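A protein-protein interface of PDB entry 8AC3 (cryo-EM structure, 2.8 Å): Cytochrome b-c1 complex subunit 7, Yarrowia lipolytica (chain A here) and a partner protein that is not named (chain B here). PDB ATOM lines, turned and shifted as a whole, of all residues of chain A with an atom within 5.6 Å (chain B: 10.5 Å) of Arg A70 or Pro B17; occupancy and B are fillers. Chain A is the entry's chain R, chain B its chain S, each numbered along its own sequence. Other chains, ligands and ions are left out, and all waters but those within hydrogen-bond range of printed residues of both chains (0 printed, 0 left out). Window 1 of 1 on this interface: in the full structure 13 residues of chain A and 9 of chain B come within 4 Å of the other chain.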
ATOM      1  N   ASN A  45     -19.928   2.938  -4.754  1.00  0.00           N
ATOM      2  CA  ASN A  45     -19.062   2.583  -5.868  1.00  0.00           C
ATOM      3  C   ASN A  45     -19.840   2.357  -7.158  1.00  0.00           C
ATOM      4  O   ASN A  45     -19.255   2.438  -8.231  1.00  0.00           O
ATOM      5  CB  ASN A  45     -18.226   1.342  -5.596  1.00  0.00           C
ATOM      6  CG  ASN A  45     -17.045   1.590  -4.684  1.00  0.00           C
ATOM      7  OD1 ASN A  45     -16.261   0.681  -4.450  1.00  0.00           O
ATOM      8  ND2 ASN A  45     -16.918   2.781  -4.121  1.00  0.00           N
ATOM      9  N   ASP A  46     -21.146   2.082  -7.058  1.00  0.00           N
ATOM     10  CA  ASP A  46     -21.987   1.929  -8.234  1.00  0.00           C
ATOM     11  C   ASP A  46     -22.036   3.209  -9.063  1.00  0.00           C
ATOM     12  O   ASP A  46     -22.340   3.157 -10.251  1.00  0.00           O
ATOM     13  CB  ASP A  46     -23.411   1.528  -7.870  1.00  0.00           C
ATOM     14  CG  ASP A  46     -23.520   0.226  -7.099  1.00  0.00           C
ATOM     15  OD1 ASP A  46     -22.688  -0.675  -7.329  1.00  0.00           O
ATOM     16  OD2 ASP A  46     -24.435   0.134  -6.255  1.00  0.00           O
ATOM     17  N   ILE A  48     -19.485   5.285  -9.812  1.00  0.00           N
ATOM     18  CA  ILE A  48     -18.245   5.714 -10.438  1.00  0.00           C
ATOM     19  C   ILE A  48     -18.304   5.489 -11.949  1.00  0.00           C
ATOM     20  O   ILE A  48     -18.715   4.418 -12.390  1.00  0.00           O
ATOM     21  CB  ILE A  48     -17.080   4.955  -9.786  1.00  0.00           C
ATOM     22  CG1 ILE A  48     -16.869   5.430  -8.350  1.00  0.00           C
ATOM     23  CG2 ILE A  48     -15.813   5.064 -10.620  1.00  0.00           C
ATOM     24  CD1 ILE A  48     -16.089   4.464  -7.508  1.00  0.00           C
ATOM     25  N   GLU A  50     -17.706   4.478 -15.569  1.00  0.00           N
ATOM     26  CA  GLU A  50     -17.090   3.220 -15.936  1.00  0.00           C
ATOM     27  C   GLU A  50     -16.650   3.198 -17.399  1.00  0.00           C
ATOM     28  O   GLU A  50     -16.066   2.211 -17.829  1.00  0.00           O
ATOM     29  CB  GLU A  50     -18.069   2.090 -15.651  1.00  0.00           C
ATOM     30  CG  GLU A  50     -19.184   2.102 -16.671  1.00  0.00           C
ATOM     31  CD  GLU A  50     -19.985   0.822 -16.808  1.00  0.00           C
ATOM     32  OE1 GLU A  50     -19.814   0.136 -17.841  1.00  0.00           O
ATOM     33  OE2 GLU A  50     -20.790   0.519 -15.897  1.00  0.00           O
ATOM     34  N   LEU A  59     -13.869  -3.711 -13.744  1.00  0.00           N
ATOM     35  CA  LEU A  59     -15.158  -4.364 -13.595  1.00  0.00           C
ATOM     36  C   LEU A  59     -15.075  -5.830 -14.001  1.00  0.00           C
ATOM     37  O   LEU A  59     -15.771  -6.661 -13.414  1.00  0.00           O
ATOM     38  CB  LEU A  59     -16.224  -3.606 -14.379  1.00  0.00           C
ATOM     39  CG  LEU A  59     -16.660  -2.298 -13.721  1.00  0.00           C
ATOM     40  CD1 LEU A  59     -17.457  -1.444 -14.689  1.00  0.00           C
ATOM     41  CD2 LEU A  59     -17.446  -2.555 -12.442  1.00  0.00           C
ATOM     42  N   LEU A  62     -13.983  -8.051 -11.088  1.00  0.00           N
ATOM     43  CA  LEU A  62     -14.875  -8.308  -9.970  1.00  0.00           C
ATOM     44  C   LEU A  62     -15.172  -9.797  -9.846  1.00  0.00           C
ATOM     45  O   LEU A  62     -15.372 -10.476 -10.851  1.00  0.00           O
ATOM     46  CB  LEU A  62     -16.191  -7.577 -10.213  1.00  0.00           C
ATOM     47  CG  LEU A  62     -16.240  -6.124  -9.760  1.00  0.00           C
ATOM     48  CD1 LEU A  62     -17.664  -5.606  -9.912  1.00  0.00           C
ATOM     49  CD2 LEU A  62     -15.762  -6.002  -8.315  1.00  0.00           C
ATOM     50  N   THR A  65     -20.071 -13.085  -8.176  1.00  0.00           N
ATOM     51  CA  THR A  65     -21.147 -12.751  -7.268  1.00  0.00           C
ATOM     52  C   THR A  65     -21.299 -11.238  -7.142  1.00  0.00           C
ATOM     53  O   THR A  65     -22.407 -10.728  -7.245  1.00  0.00           O
ATOM     54  CB  THR A  65     -20.884 -13.377  -5.898  1.00  0.00           C
ATOM     55  OG1 THR A  65     -20.740 -14.785  -6.086  1.00  0.00           O
ATOM     56  CG2 THR A  65     -21.992 -13.109  -4.905  1.00  0.00           C
ATOM     57  N   GLU A  66     -20.191 -10.542  -6.873  1.00  0.00           N
ATOM     58  CA  GLU A  66     -20.199  -9.093  -6.744  1.00  0.00           C
ATOM     59  C   GLU A  66     -20.693  -8.459  -8.038  1.00  0.00           C
ATOM     60  O   GLU A  66     -21.425  -7.472  -8.026  1.00  0.00           O
ATOM     61  CB  GLU A  66     -18.811  -8.560  -6.390  1.00  0.00           C
ATOM     62  CG  GLU A  66     -18.402  -8.870  -4.965  1.00  0.00           C
ATOM     63  CD  GLU A  66     -18.781  -7.853  -3.897  1.00  0.00           C
ATOM     64  OE1 GLU A  66     -18.022  -7.737  -2.914  1.00  0.00           O
ATOM     65  OE2 GLU A  66     -19.835  -7.189  -4.036  1.00  0.00           O
ATOM     66  N   SER A  67     -20.274  -9.038  -9.155  1.00  0.00           N
ATOM     67  CA  SER A  67     -20.668  -8.493 -10.429  1.00  0.00           C
ATOM     68  C   SER A  67     -22.172  -8.656 -10.644  1.00  0.00           C
ATOM     69  O   SER A  67     -22.805  -7.729 -11.148  1.00  0.00           O
ATOM     70  CB  SER A  67     -19.902  -9.141 -11.513  1.00  0.00           C
ATOM     71  OG  SER A  67     -20.196  -8.503 -12.745  1.00  0.00           O
ATOM     72  N   TYR A  68     -22.714  -9.837 -10.306  1.00  0.00           N
ATOM     73  CA  TYR A  68     -24.122 -10.109 -10.527  1.00  0.00           C
ATOM     74  C   TYR A  68     -24.958  -9.196  -9.651  1.00  0.00           C
ATOM     75  O   TYR A  68     -26.010  -8.741 -10.092  1.00  0.00           O
ATOM     76  CB  TYR A  68     -24.513 -11.544 -10.186  1.00  0.00           C
ATOM     77  CG  TYR A  68     -23.991 -12.561 -11.159  1.00  0.00           C
ATOM     78  CD1 TYR A  68     -24.109 -12.373 -12.527  1.00  0.00           C
ATOM     79  CD2 TYR A  68     -23.371 -13.713 -10.709  1.00  0.00           C
ATOM     80  CE1 TYR A  68     -23.635 -13.312 -13.431  1.00  0.00           C
ATOM     81  CE2 TYR A  68     -22.878 -14.656 -11.597  1.00  0.00           C
ATOM     82  CZ  TYR A  68     -23.014 -14.458 -12.962  1.00  0.00           C
ATOM     83  OH  TYR A  68     -22.534 -15.392 -13.833  1.00  0.00           O
ATOM     84  N   ASP A  69     -24.461  -8.927  -8.439  1.00  0.00           N
ATOM     85  CA  ASP A  69     -25.197  -8.084  -7.518  1.00  0.00           C
ATOM     86  C   ASP A  69     -25.221  -6.647  -8.015  1.00  0.00           C
ATOM     87  O   ASP A  69     -26.199  -5.932  -7.802  1.00  0.00           O
ATOM     88  CB  ASP A  69     -24.590  -8.115  -6.123  1.00  0.00           C
ATOM     89  CG  ASP A  69     -24.814  -9.422  -5.387  1.00  0.00           C
ATOM     90  OD1 ASP A  69     -25.562 -10.278  -5.910  1.00  0.00           O
ATOM     91  OD2 ASP A  69     -24.232  -9.581  -4.289  1.00  0.00           O
ATOM     92  N   ARG A  70     -24.106  -6.213  -8.600  1.00  0.00           N
ATOM     93  CA  ARG A  70     -24.026  -4.855  -9.094  1.00  0.00           C
ATOM     94  C   ARG A  70     -25.049  -4.683 -10.211  1.00  0.00           C
ATOM     95  O   ARG A  70     -25.760  -3.682 -10.245  1.00  0.00           O
ATOM     96  CB  ARG A  70     -22.590  -4.558  -9.539  1.00  0.00           C
ATOM     97  CG  ARG A  70     -22.418  -3.265 -10.324  1.00  0.00           C
ATOM     98  CD  ARG A  70     -20.974  -2.910 -10.618  1.00  0.00           C
ATOM     99  NE  ARG A  70     -20.849  -1.707 -11.431  1.00  0.00           N
ATOM    100  CZ  ARG A  70     -20.971  -1.682 -12.754  1.00  0.00           C
ATOM    101  NH1 ARG A  70     -20.844  -0.537 -13.401  1.00  0.00           N
ATOM    102  NH2 ARG A  70     -21.228  -2.792 -13.428  1.00  0.00           N
ATOM    103  N   VAL A  71     -25.140  -5.672 -11.102  1.00  0.00           N
ATOM    104  CA  VAL A  71     -26.079  -5.561 -12.203  1.00  0.00           C
ATOM    105  C   VAL A  71     -27.492  -5.432 -11.649  1.00  0.00           C
ATOM    106  O   VAL A  71     -28.247  -4.569 -12.074  1.00  0.00           O
ATOM    107  CB  VAL A  71     -25.956  -6.725 -13.191  1.00  0.00           C
ATOM    108  CG1 VAL A  71     -27.210  -6.867 -14.036  1.00  0.00           C
ATOM    109  CG2 VAL A  71     -24.749  -6.527 -14.087  1.00  0.00           C
ATOM    110  N   TYR A  72     -27.825  -6.223 -10.642  1.00  0.00           N
ATOM    111  CA  TYR A  72     -29.136  -6.051 -10.055  1.00  0.00           C
ATOM    112  C   TYR A  72     -29.348  -4.661  -9.446  1.00  0.00           C
ATOM    113  O   TYR A  72     -30.395  -4.060  -9.660  1.00  0.00           O
ATOM    114  CB  TYR A  72     -29.416  -7.151  -9.047  1.00  0.00           C
ATOM    115  CG  TYR A  72     -30.720  -6.936  -8.342  1.00  0.00           C
ATOM    116  CD1 TYR A  72     -31.918  -6.974  -9.042  1.00  0.00           C
ATOM    117  CD2 TYR A  72     -30.754  -6.635  -6.990  1.00  0.00           C
ATOM    118  CE1 TYR A  72     -33.126  -6.751  -8.402  1.00  0.00           C
ATOM    119  CE2 TYR A  72     -31.957  -6.440  -6.330  1.00  0.00           C
ATOM    120  CZ  TYR A  72     -33.147  -6.486  -7.042  1.00  0.00           C
ATOM    121  OH  TYR A  72     -34.341  -6.281  -6.407  1.00  0.00           O
ATOM    122  N   ARG A  73     -28.386  -4.138  -8.679  1.00  0.00           N
ATOM    123  CA  ARG A  73     -28.570  -2.803  -8.124  1.00  0.00           C
ATOM    124  C   ARG A  73     -28.759  -1.748  -9.214  1.00  0.00           C
ATOM    125  O   ARG A  73     -29.551  -0.829  -9.037  1.00  0.00           O
ATOM    126  CB  ARG A  73     -27.423  -2.395  -7.204  1.00  0.00           C
ATOM    127  CG  ARG A  73     -27.427  -3.106  -5.863  1.00  0.00           C
ATOM    128  CD  ARG A  73     -26.388  -2.559  -4.903  1.00  0.00           C
ATOM    129  NE  ARG A  73     -25.073  -2.425  -5.498  1.00  0.00           N
ATOM    130  CZ  ARG A  73     -24.165  -3.390  -5.574  1.00  0.00           C
ATOM    131  NH1 ARG A  73     -23.015  -3.138  -6.167  1.00  0.00           N
ATOM    132  NH2 ARG A  73     -24.405  -4.595  -5.080  1.00  0.00           N
ATOM    133  N   LEU A  74     -28.046  -1.862 -10.336  1.00  0.00           N
ATOM    134  CA  LEU A  74     -28.216  -0.855 -11.370  1.00  0.00           C
ATOM    135  C   LEU A  74     -29.598  -0.956 -11.996  1.00  0.00           C
ATOM    136  O   LEU A  74     -30.215   0.076 -12.270  1.00  0.00           O
ATOM    137  CB  LEU A  74     -27.132  -0.987 -12.437  1.00  0.00           C
ATOM    138  CG  LEU A  74     -25.695  -0.798 -11.958  1.00  0.00           C
ATOM    139  CD1 LEU A  74     -24.747  -0.911 -13.138  1.00  0.00           C
ATOM    140  CD2 LEU A  74     -25.504   0.533 -11.245  1.00  0.00           C
ATOM    141  N   ILE A  75     -30.076  -2.187 -12.188  1.00  0.00           N
ATOM    142  CA  ILE A  75     -31.350  -2.354 -12.863  1.00  0.00           C
ATOM    143  C   ILE A  75     -32.462  -1.892 -11.936  1.00  0.00           C
ATOM    144  O   ILE A  75     -33.350  -1.163 -12.348  1.00  0.00           O
ATOM    145  CB  ILE A  75     -31.558  -3.801 -13.295  1.00  0.00           C
ATOM    146  CG1 ILE A  75     -30.717  -4.074 -14.533  1.00  0.00           C
ATOM    147  CG2 ILE A  75     -33.028  -4.104 -13.523  1.00  0.00           C
ATOM    148  CD1 ILE A  75     -30.581  -5.535 -14.819  1.00  0.00           C
ATOM    149  N   TYR A 101     -16.626  -2.107  -2.768  1.00  0.00           N
ATOM    150  CA  TYR A 101     -16.336  -3.412  -3.332  1.00  0.00           C
ATOM    151  C   TYR A 101     -15.409  -3.220  -4.528  1.00  0.00           C
ATOM    152  O   TYR A 101     -14.670  -4.123  -4.880  1.00  0.00           O
ATOM    153  CB  TYR A 101     -17.622  -4.169  -3.688  1.00  0.00           C
ATOM    154  CG  TYR A 101     -18.382  -3.481  -4.786  1.00  0.00           C
ATOM    155  CD1 TYR A 101     -18.091  -3.737  -6.120  1.00  0.00           C
ATOM    156  CD2 TYR A 101     -19.325  -2.502  -4.496  1.00  0.00           C
ATOM    157  CE1 TYR A 101     -18.745  -3.059  -7.142  1.00  0.00           C
ATOM    158  CE2 TYR A 101     -19.985  -1.814  -5.508  1.00  0.00           C
ATOM    159  CZ  TYR A 101     -19.691  -2.089  -6.838  1.00  0.00           C
ATOM    160  OH  TYR A 101     -20.303  -1.392  -7.847  1.00  0.00           O
ATOM    161  N   LEU A 102     -15.436  -2.040  -5.143  1.00  0.00           N
ATOM    162  CA  LEU A 102     -14.746  -1.893  -6.407  1.00  0.00           C
ATOM    163  C   LEU A 102     -13.414  -1.187  -6.223  1.00  0.00           C
ATOM    164  O   LEU A 102     -12.516  -1.390  -7.032  1.00  0.00           O
ATOM    165  CB  LEU A 102     -15.641  -1.122  -7.368  1.00  0.00           C
ATOM    166  CG  LEU A 102     -15.111  -0.979  -8.787  1.00  0.00           C
ATOM    167  CD1 LEU A 102     -15.043  -2.328  -9.488  1.00  0.00           C
ATOM    168  CD2 LEU A 102     -15.990  -0.021  -9.556  1.00  0.00           C
ATOM    169  N   TYR B   7     -18.262   1.163 -26.371  1.00  0.00           N
ATOM    170  CA  TYR B   7     -18.921   1.365 -24.970  1.00  0.00           C
ATOM    171  C   TYR B   7     -20.430   1.114 -24.946  1.00  0.00           C
ATOM    172  O   TYR B   7     -21.039   0.958 -23.881  1.00  0.00           O
ATOM    173  CB  TYR B   7     -18.695   2.764 -24.392  1.00  0.00           C
ATOM    174  CG  TYR B   7     -17.306   2.997 -23.865  1.00  0.00           C
ATOM    175  CD1 TYR B   7     -16.764   2.205 -22.857  1.00  0.00           C
ATOM    176  CD2 TYR B   7     -16.510   3.996 -24.408  1.00  0.00           C
ATOM    177  CE1 TYR B   7     -15.466   2.399 -22.405  1.00  0.00           C
ATOM    178  CE2 TYR B   7     -15.214   4.207 -23.961  1.00  0.00           C
ATOM    179  CZ  TYR B   7     -14.692   3.409 -22.954  1.00  0.00           C
ATOM    180  OH  TYR B   7     -13.418   3.619 -22.507  1.00  0.00           O
ATOM    181  N   GLY B   9     -22.963  -1.553 -27.289  1.00  0.00           N
ATOM    182  CA  GLY B   9     -23.056  -2.428 -28.441  1.00  0.00           C
ATOM    183  C   GLY B   9     -24.382  -2.260 -29.168  1.00  0.00           C
ATOM    184  O   GLY B   9     -24.769  -1.169 -29.580  1.00  0.00           O
ATOM    185  N   GLY B  12     -28.382  -7.872 -28.279  1.00  0.00           N
ATOM    186  CA  GLY B  12     -27.669  -9.128 -28.355  1.00  0.00           C
ATOM    187  C   GLY B  12     -26.275  -9.011 -27.757  1.00  0.00           C
ATOM    188  O   GLY B  12     -25.797  -9.968 -27.150  1.00  0.00           O
ATOM    189  N   HIS B  13     -25.633  -7.848 -27.919  1.00  0.00           N
ATOM    190  CA  HIS B  13     -24.287  -7.675 -27.400  1.00  0.00           C
ATOM    191  C   HIS B  13     -24.115  -6.246 -26.892  1.00  0.00           C
ATOM    192  O   HIS B  13     -23.212  -5.531 -27.317  1.00  0.00           O
ATOM    193  CB  HIS B  13     -23.269  -8.129 -28.457  1.00  0.00           C
ATOM    194  CG  HIS B  13     -23.379  -7.353 -29.726  1.00  0.00           C
ATOM    195  ND1 HIS B  13     -24.387  -7.576 -30.644  1.00  0.00           N
ATOM    196  CD2 HIS B  13     -22.634  -6.336 -30.214  1.00  0.00           C
ATOM    197  CE1 HIS B  13     -24.253  -6.738 -31.652  1.00  0.00           C
ATOM    198  NE2 HIS B  13     -23.187  -5.960 -31.409  1.00  0.00           N
ATOM    199  N   MET B  14     -24.989  -5.846 -25.967  1.00  0.00           N
ATOM    200  CA  MET B  14     -25.094  -4.453 -25.574  1.00  0.00           C
ATOM    201  C   MET B  14     -23.874  -4.037 -24.759  1.00  0.00           C
ATOM    202  O   MET B  14     -23.492  -2.875 -24.784  1.00  0.00           O
ATOM    203  CB  MET B  14     -26.343  -4.219 -24.725  1.00  0.00           C
ATOM    204  CG  MET B  14     -26.760  -2.762 -24.661  1.00  0.00           C
ATOM    205  SD  MET B  14     -27.311  -2.185 -26.286  1.00  0.00           S
ATOM    206  CE  MET B  14     -28.770  -3.208 -26.481  1.00  0.00           C
ATOM    207  N   GLY B  15     -23.258  -4.982 -24.050  1.00  0.00           N
ATOM    208  CA  GLY B  15     -22.071  -4.646 -23.284  1.00  0.00           C
ATOM    209  C   GLY B  15     -22.357  -4.587 -21.789  1.00  0.00           C
ATOM    210  O   GLY B  15     -21.562  -4.047 -21.019  1.00  0.00           O
ATOM    211  N   SER B  16     -23.483  -5.181 -21.385  1.00  0.00           N
ATOM    212  CA  SER B  16     -23.766  -5.444 -19.984  1.00  0.00           C
ATOM    213  C   SER B  16     -22.760  -6.460 -19.444  1.00  0.00           C
ATOM    214  O   SER B  16     -22.335  -7.364 -20.166  1.00  0.00           O
ATOM    215  CB  SER B  16     -25.179  -5.931 -19.830  1.00  0.00           C
ATOM    216  OG  SER B  16     -25.465  -6.305 -18.488  1.00  0.00           O
ATOM    217  N   PRO B  17     -22.347  -6.353 -18.162  1.00  0.00           N
ATOM    218  CA  PRO B  17     -21.722  -7.483 -17.478  1.00  0.00           C
ATOM    219  C   PRO B  17     -22.734  -8.623 -17.531  1.00  0.00           C
ATOM    220  O   PRO B  17     -23.928  -8.375 -17.671  1.00  0.00           O
ATOM    221  CB  PRO B  17     -21.680  -6.995 -16.033  1.00  0.00           C
ATOM    222  CG  PRO B  17     -21.576  -5.515 -16.160  1.00  0.00           C
ATOM    223  CD  PRO B  17     -22.484  -5.164 -17.310  1.00  0.00           C
ATOM    224  N   PRO B  18     -22.316  -9.901 -17.439  1.00  0.00           N
ATOM    225  CA  PRO B  18     -23.269 -11.004 -17.561  1.00  0.00           C
ATOM    226  C   PRO B  18     -24.348 -10.911 -16.487  1.00  0.00           C
ATOM    227  O   PRO B  18     -24.071 -10.599 -15.327  1.00  0.00           O
ATOM    228  CB  PRO B  18     -22.382 -12.235 -17.379  1.00  0.00           C
ATOM    229  CG  PRO B  18     -21.022 -11.747 -17.804  1.00  0.00           C
ATOM    230  CD  PRO B  18     -20.937 -10.360 -17.211  1.00  0.00           C
ATOM    231  N   GLN B  19     -25.591 -11.099 -16.916  1.00  0.00           N
ATOM    232  CA  GLN B  19     -26.712 -11.035 -16.003  1.00  0.00           C
ATOM    233  C   GLN B  19     -27.159 -12.451 -15.704  1.00  0.00           C
ATOM    234  O   GLN B  19     -27.222 -13.287 -16.594  1.00  0.00           O
ATOM    235  CB  GLN B  19     -27.860 -10.265 -16.630  1.00  0.00           C
ATOM    236  CG  GLN B  19     -27.413  -8.898 -17.081  1.00  0.00           C
ATOM    237  CD  GLN B  19     -28.595  -8.005 -17.351  1.00  0.00           C
ATOM    238  OE1 GLN B  19     -29.726  -8.308 -16.960  1.00  0.00           O
ATOM    239  NE2 GLN B  19     -28.334  -6.891 -18.025  1.00  0.00           N
ATOM    240  N   LYS B  20     -27.426 -12.714 -14.436  1.00  0.00           N
ATOM    241  CA  LYS B  20     -27.966 -13.988 -14.034  1.00  0.00           C
ATOM    242  C   LYS B  20     -28.742 -13.726 -12.757  1.00  0.00           C
ATOM    243  O   LYS B  20     -28.352 -12.885 -11.958  1.00  0.00           O
ATOM    244  CB  LYS B  20     -26.809 -14.950 -13.787  1.00  0.00           C
ATOM    245  CG  LYS B  20     -27.228 -16.382 -13.527  1.00  0.00           C
ATOM    246  CD  LYS B  20     -26.087 -17.348 -13.721  1.00  0.00           C
ATOM    247  CE  LYS B  20     -26.362 -18.711 -13.121  1.00  0.00           C
ATOM    248  NZ  LYS B  20     -25.112 -19.497 -12.980  1.00  0.00           N
ATOM    249  N   GLY B  21     -29.867 -14.412 -12.577  1.00  0.00           N
ATOM    250  CA  GLY B  21     -30.502 -14.363 -11.278  1.00  0.00           C
ATOM    251  C   GLY B  21     -31.599 -13.306 -11.153  1.00  0.00           C
ATOM    252  O   GLY B  21     -32.303 -13.298 -10.143  1.00  0.00           O
ATOM    253  N   ILE B  22     -31.812 -12.471 -12.174  1.00  0.00           N
ATOM    254  CA  ILE B  22     -32.913 -11.528 -12.080  1.00  0.00           C
ATOM    255  C   ILE B  22     -34.085 -12.029 -12.912  1.00  0.00           C
ATOM    256  O   ILE B  22     -33.930 -12.259 -14.107  1.00  0.00           O
ATOM    257  CB  ILE B  22     -32.484 -10.134 -12.545  1.00  0.00           C
ATOM    258  CG1 ILE B  22     -31.183  -9.683 -11.877  1.00  0.00           C
ATOM    259  CG2 ILE B  22     -33.618  -9.155 -12.309  1.00  0.00           C
ATOM    260  CD1 ILE B  22     -30.514  -8.512 -12.565  1.00  0.00           C
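Asp A46 touches none of the printed residues of chain B. Printed residues of chain B within 4 Å of Tyr A68: Pro B18 and Lys B20. Asp A69 touches none of the printed residues of chain B. Printed residues of chain B within 4 Å of Tyr A72: Ile B22 (3.8 Å). No residue of chain B comes within 4 Å of Leu A74. Printed residues of chain A within 4 Å of Pro B17: Ser A67 (3.9 Å), Arg A70 (3.9 Å) and Val A71 (3.7 Å). Of the printed residues of chain A, Gln B19 touches Val A71 (3.7 Å) and Ile A75 (3.6 Å). Printed residues of chain A within 4 Å of Ile B22: Val A71 (3.97 Å), Tyr A72 (3.8 Å) and Ile A75 (3.7 Å). The nearest residue of chain B that does not touch Arg A70 is Ile B22 (7.1 Å). The nearest printed residue of chain A that does not touch Pro B17 is Leu A59 (6.0 Å). The nearest printed residue of chain A that does not touch Lys B20 is Val A71 (5.9 Å).
Printed residues of chain B that touch a printed residue of chain A: Pro B17, Pro B18, Gln B19, Lys B20 and Ile B22. Hydrophobic or aromatic side chains of chain B within 4 Å of the printed part of chain A: Pro B17 and Ile B22. Of the 19 printed residues of chain A, 6 touch a printed residue of chain B. Hydrophobic or aromatic side chains of chain A within 4 Å of the printed part of chain B: Tyr A68, Val A71, Tyr A72 and Ile A75. Among the printed residues, no Asp or Glu carboxylate lies within 4 Å of a Lys or Arg side-chain nitrogen of the other chain.
Pro B17 touches Ser A67. CD1 of Tyr A68 touches O of Pro B18 (3.3 Å). Lys B20 touches Tyr A68. CG of Pro B17 touches NH2 of Arg A70, at 3.9 Å. Pro B17 touches Val A71. Val A71 touches Gln B19 (CG1 to CG, 3.7 Å). CG1 of Val A71 touches CD1 of Ile B22, at 3.97 Å. Tyr A72 touches Ile B22. Ile A75 touches Gln B19 (CD1 to OE1, 3.6 Å). Ile A75 touches Ile B22.
The guanidinium group of Arg A70 lies within salt-bridge range of the side-chain carboxylate of Glu A50 (2.7 Å). The side-chain hydroxyl of Ser B16 lies within hydrogen-bond range of the side-chain amide nitrogen of Gln B19 (3.0 Å).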
